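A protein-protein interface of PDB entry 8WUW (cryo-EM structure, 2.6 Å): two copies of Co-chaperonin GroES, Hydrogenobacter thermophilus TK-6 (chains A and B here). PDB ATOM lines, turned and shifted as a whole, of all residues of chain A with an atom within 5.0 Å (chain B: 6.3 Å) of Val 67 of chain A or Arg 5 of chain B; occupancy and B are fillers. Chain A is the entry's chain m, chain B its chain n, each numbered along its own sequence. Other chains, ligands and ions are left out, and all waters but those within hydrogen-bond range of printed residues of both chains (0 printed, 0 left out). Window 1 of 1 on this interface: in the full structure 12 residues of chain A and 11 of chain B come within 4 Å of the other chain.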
ATOM      1  N   ILE A  11      -2.055  13.487  13.360  1.00  0.00           N
ATOM      2  CA  ILE A  11      -1.915  14.125  14.665  1.00  0.00           C
ATOM      3  C   ILE A  11      -2.771  13.366  15.670  1.00  0.00           C
ATOM      4  O   ILE A  11      -3.927  13.036  15.382  1.00  0.00           O
ATOM      5  CB  ILE A  11      -2.321  15.611  14.624  1.00  0.00           C
ATOM      6  CG1 ILE A  11      -1.502  16.365  13.576  1.00  0.00           C
ATOM      7  CG2 ILE A  11      -2.139  16.255  15.991  1.00  0.00           C
ATOM      8  CD1 ILE A  11      -0.035  16.472  13.917  1.00  0.00           C
ATOM      9  N   VAL A  61       3.733  21.478  12.531  1.00  0.00           N
ATOM     10  CA  VAL A  61       3.701  21.172  13.955  1.00  0.00           C
ATOM     11  C   VAL A  61       4.824  20.198  14.278  1.00  0.00           C
ATOM     12  O   VAL A  61       5.136  19.298  13.490  1.00  0.00           O
ATOM     13  CB  VAL A  61       2.327  20.607  14.365  1.00  0.00           C
ATOM     14  CG1 VAL A  61       1.270  21.697  14.304  1.00  0.00           C
ATOM     15  CG2 VAL A  61       1.944  19.447  13.465  1.00  0.00           C
ATOM     16  N   ASP A  65       4.441  19.526  20.938  1.00  0.00           N
ATOM     17  CA  ASP A  65       3.682  20.764  20.917  1.00  0.00           C
ATOM     18  C   ASP A  65       2.183  20.476  21.020  1.00  0.00           C
ATOM     19  O   ASP A  65       1.725  19.360  20.774  1.00  0.00           O
ATOM     20  CB  ASP A  65       3.976  21.557  19.640  1.00  0.00           C
ATOM     21  CG  ASP A  65       3.556  20.822  18.382  1.00  0.00           C
ATOM     22  OD1 ASP A  65       3.232  19.619  18.471  1.00  0.00           O
ATOM     23  OD2 ASP A  65       3.550  21.462  17.306  1.00  0.00           O
ATOM     24  N   LYS A  66       1.425  21.505  21.380  1.00  0.00           N
ATOM     25  CA  LYS A  66      -0.024  21.417  21.426  1.00  0.00           C
ATOM     26  C   LYS A  66      -0.635  22.323  20.362  1.00  0.00           C
ATOM     27  O   LYS A  66      -0.370  23.532  20.323  1.00  0.00           O
ATOM     28  CB  LYS A  66      -0.552  21.773  22.827  1.00  0.00           C
ATOM     29  CG  LYS A  66       0.131  22.956  23.549  1.00  0.00           C
ATOM     30  CD  LYS A  66      -0.227  22.865  25.031  1.00  0.00           C
ATOM     31  CE  LYS A  66       0.541  23.801  25.936  1.00  0.00           C
ATOM     32  NZ  LYS A  66       0.277  23.483  27.373  1.00  0.00           N
ATOM     33  N   VAL A  67      -1.475  21.732  19.516  1.00  0.00           N
ATOM     34  CA  VAL A  67      -2.124  22.427  18.416  1.00  0.00           C
ATOM     35  C   VAL A  67      -3.479  22.938  18.883  1.00  0.00           C
ATOM     36  O   VAL A  67      -4.194  22.268  19.638  1.00  0.00           O
ATOM     37  CB  VAL A  67      -2.282  21.515  17.182  1.00  0.00           C
ATOM     38  CG1 VAL A  67      -2.939  20.201  17.578  1.00  0.00           C
ATOM     39  CG2 VAL A  67      -3.090  22.202  16.101  1.00  0.00           C
ATOM     40  N   VAL A  68      -3.812  24.162  18.476  1.00  0.00           N
ATOM     41  CA  VAL A  68      -5.146  24.672  18.738  1.00  0.00           C
ATOM     42  C   VAL A  68      -6.137  24.072  17.752  1.00  0.00           C
ATOM     43  O   VAL A  68      -5.960  24.124  16.526  1.00  0.00           O
ATOM     44  CB  VAL A  68      -5.150  26.200  18.707  1.00  0.00           C
ATOM     45  CG1 VAL A  68      -4.760  26.711  17.323  1.00  0.00           C
ATOM     46  CG2 VAL A  68      -6.515  26.721  19.146  1.00  0.00           C
ATOM     47  N   PHE A  69      -7.209  23.513  18.297  1.00  0.00           N
ATOM     48  CA  PHE A  69      -8.269  22.891  17.527  1.00  0.00           C
ATOM     49  C   PHE A  69      -9.621  23.440  17.972  1.00  0.00           C
ATOM     50  O   PHE A  69      -9.806  23.807  19.136  1.00  0.00           O
ATOM     51  CB  PHE A  69      -8.207  21.382  17.673  1.00  0.00           C
ATOM     52  CG  PHE A  69      -7.668  20.922  18.987  1.00  0.00           C
ATOM     53  CD1 PHE A  69      -8.409  21.100  20.130  1.00  0.00           C
ATOM     54  CD2 PHE A  69      -6.462  20.242  19.074  1.00  0.00           C
ATOM     55  CE1 PHE A  69      -7.945  20.644  21.348  1.00  0.00           C
ATOM     56  CE2 PHE A  69      -6.003  19.779  20.292  1.00  0.00           C
ATOM     57  CZ  PHE A  69      -6.746  19.981  21.429  1.00  0.00           C
ATOM     58  N   MET A  87      -6.880  13.804  15.454  1.00  0.00           N
ATOM     59  CA  MET A  87      -7.175  14.884  14.521  1.00  0.00           C
ATOM     60  C   MET A  87      -6.192  14.842  13.358  1.00  0.00           C
ATOM     61  O   MET A  87      -5.462  13.861  13.189  1.00  0.00           O
ATOM     62  CB  MET A  87      -7.119  16.260  15.200  1.00  0.00           C
ATOM     63  CG  MET A  87      -5.873  16.538  16.037  1.00  0.00           C
ATOM     64  SD  MET A  87      -5.403  15.242  17.195  1.00  0.00           S
ATOM     65  CE  MET A  87      -6.812  15.265  18.301  1.00  0.00           C
ATOM     66  N   MET B   1       5.118  28.963  23.910  1.00  0.00           N
ATOM     67  CA  MET B   1       4.420  28.880  22.632  1.00  0.00           C
ATOM     68  C   MET B   1       2.948  29.236  22.796  1.00  0.00           C
ATOM     69  O   MET B   1       2.274  28.736  23.699  1.00  0.00           O
ATOM     70  CB  MET B   1       4.566  27.481  22.032  1.00  0.00           C
ATOM     71  CG  MET B   1       3.458  27.095  21.067  1.00  0.00           C
ATOM     72  SD  MET B   1       2.243  25.999  21.819  1.00  0.00           S
ATOM     73  CE  MET B   1       3.000  24.410  21.511  1.00  0.00           C
ATOM     74  N   ALA B   2       2.455  30.108  21.921  1.00  0.00           N
ATOM     75  CA  ALA B   2       1.067  30.534  21.985  1.00  0.00           C
ATOM     76  C   ALA B   2       0.155  29.463  21.392  1.00  0.00           C
ATOM     77  O   ALA B   2       0.597  28.518  20.736  1.00  0.00           O
ATOM     78  CB  ALA B   2       0.881  31.862  21.252  1.00  0.00           C
ATOM     79  N   ARG B   3      -1.145  29.622  21.639  1.00  0.00           N
ATOM     80  CA  ARG B   3      -2.116  28.669  21.114  1.00  0.00           C
ATOM     81  C   ARG B   3      -2.106  28.659  19.587  1.00  0.00           C
ATOM     82  O   ARG B   3      -2.281  27.610  18.964  1.00  0.00           O
ATOM     83  CB  ARG B   3      -3.505  28.990  21.667  1.00  0.00           C
ATOM     84  CG  ARG B   3      -4.437  27.792  21.761  1.00  0.00           C
ATOM     85  CD  ARG B   3      -3.789  26.596  22.440  1.00  0.00           C
ATOM     86  NE  ARG B   3      -4.721  25.479  22.552  1.00  0.00           N
ATOM     87  CZ  ARG B   3      -4.381  24.203  22.427  1.00  0.00           C
ATOM     88  NH1 ARG B   3      -3.140  23.841  22.147  1.00  0.00           N
ATOM     89  NH2 ARG B   3      -5.313  23.267  22.577  1.00  0.00           N
ATOM     90  N   LEU B   4      -1.906  29.821  18.970  1.00  0.00           N
ATOM     91  CA  LEU B   4      -1.891  29.959  17.515  1.00  0.00           C
ATOM     92  C   LEU B   4      -0.494  29.650  16.984  1.00  0.00           C
ATOM     93  O   LEU B   4       0.456  30.388  17.234  1.00  0.00           O
ATOM     94  CB  LEU B   4      -2.342  31.359  17.122  1.00  0.00           C
ATOM     95  CG  LEU B   4      -2.530  31.614  15.630  1.00  0.00           C
ATOM     96  CD1 LEU B   4      -3.526  30.642  15.042  1.00  0.00           C
ATOM     97  CD2 LEU B   4      -2.974  33.040  15.400  1.00  0.00           C
ATOM     98  N   ARG B   5      -0.348  28.540  16.264  1.00  0.00           N
ATOM     99  CA  ARG B   5       0.973  28.121  15.823  1.00  0.00           C
ATOM    100  C   ARG B   5       1.342  28.887  14.558  1.00  0.00           C
ATOM    101  O   ARG B   5       0.474  29.451  13.892  1.00  0.00           O
ATOM    102  CB  ARG B   5       1.056  26.618  15.522  1.00  0.00           C
ATOM    103  CG  ARG B   5       0.803  25.685  16.692  1.00  0.00           C
ATOM    104  CD  ARG B   5      -0.704  25.688  16.951  1.00  0.00           C
ATOM    105  NE  ARG B   5      -1.348  25.117  15.758  1.00  0.00           N
ATOM    106  CZ  ARG B   5      -2.220  25.728  14.969  1.00  0.00           C
ATOM    107  NH1 ARG B   5      -2.523  27.005  15.144  1.00  0.00           N
ATOM    108  NH2 ARG B   5      -2.769  25.042  13.963  1.00  0.00           N
ATOM    109  N   PRO B   6       2.621  28.906  14.189  1.00  0.00           N
ATOM    110  CA  PRO B   6       2.988  29.407  12.857  1.00  0.00           C
ATOM    111  C   PRO B   6       2.463  28.480  11.770  1.00  0.00           C
ATOM    112  O   PRO B   6       2.944  27.357  11.603  1.00  0.00           O
ATOM    113  CB  PRO B   6       4.522  29.430  12.895  1.00  0.00           C
ATOM    114  CG  PRO B   6       4.878  29.368  14.355  1.00  0.00           C
ATOM    115  CD  PRO B   6       3.802  28.582  15.008  1.00  0.00           C
ATOM    116  N   LEU B   7       1.456  28.956  11.038  1.00  0.00           N
ATOM    117  CA  LEU B   7       0.902  28.256   9.891  1.00  0.00           C
ATOM    118  C   LEU B   7       0.996  29.179   8.683  1.00  0.00           C
ATOM    119  O   LEU B   7       1.439  30.327   8.789  1.00  0.00           O
ATOM    120  CB  LEU B   7      -0.546  27.815  10.141  1.00  0.00           C
ATOM    121  CG  LEU B   7      -1.046  26.597   9.358  1.00  0.00           C
ATOM    122  CD1 LEU B   7      -0.347  25.322   9.807  1.00  0.00           C
ATOM    123  CD2 LEU B   7      -2.559  26.468   9.467  1.00  0.00           C
ATOM    124  N   LYS B  10      -0.792  32.892   8.562  1.00  0.00           N
ATOM    125  CA  LYS B  10      -1.478  33.094   9.828  1.00  0.00           C
ATOM    126  C   LYS B  10      -1.439  34.569  10.211  1.00  0.00           C
ATOM    127  O   LYS B  10      -0.383  35.204  10.156  1.00  0.00           O
ATOM    128  CB  LYS B  10      -0.827  32.246  10.920  1.00  0.00           C
ATOM    129  CG  LYS B  10      -1.237  32.628  12.329  1.00  0.00           C
ATOM    130  CD  LYS B  10      -0.122  33.355  13.069  1.00  0.00           C
ATOM    131  CE  LYS B  10       0.961  32.400  13.523  1.00  0.00           C
ATOM    132  NZ  LYS B  10       1.968  33.041  14.407  1.00  0.00           N
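The guanidinium group (NH1) of Arg 3 of chain B is in hydrogen-bond range of the backbone carbonyl oxygen (O) of Lys 66 of chain A, at 3.3 Å. NH1 of Arg 3 of chain B sits at hydrogen-bond distance from O of Val 67 of chain A (3.1 Å).
Among the printed residues, pairs that only touch across the chains: Val 68 of chain A with Arg 3 of chain B, Val 68 of chain A with Arg 5 of chain B, Lys 66 of chain A with Met 1 of chain B, Val 67 of chain A with Arg 5 of chain B, Asp 65 of chain A with Met 1 of chain B and Phe 69 of chain A with Arg 3 of chain B.
Val 67 of chain A touches just these residues of chain B: Arg 3 (3.1 Å) and Arg 5 (3.4 Å). Of the printed residues of chain A, Arg 3 of chain B touches Lys 66 (3.3 Å), Val 67 (3.1 Å), Val 68 (3.1 Å) and Phe 69 (3.8 Å). Printed residues of chain A within 4 Å of Met 1 of chain B: Asp 65 (3.5 Å) and Lys 66 (3.3 Å). Of the printed residues of chain B, Phe 69 of chain A touches Arg 3 (3.8 Å). Printed residues of chain B within 4 Å of Lys 66 of chain A: Met 1 (3.3 Å) and Arg 3 (3.3 Å). The nearest printed residue of chain B that does not touch Phe 69 of chain A is Arg 5 of chain B (6.4 Å).
Hydrophobic or aromatic side chains of chain B that line the printed part of chain A: Met 1. Along chain B the printed residues that touch a printed residue of chain A span positions 1 to 5. Of the 8 printed residues of chain A, 5 touch a printed residue of chain B. Printed residues of chain A that touch a printed residue of chain B: Asp 65, Lys 66, Val 67, Val 68 and Phe 69. Hydrophobic or aromatic side chains of chain A that line the printed part of chain B: Val 67, Val 68 and Phe 69. Among the printed residues, 8 pairs touch across the chains. Among the printed residues, no Asp or Glu carboxylate lies within 4 Å of a Lys or Arg side-chain nitrogen of the other chain.
No position is printed for both chains.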
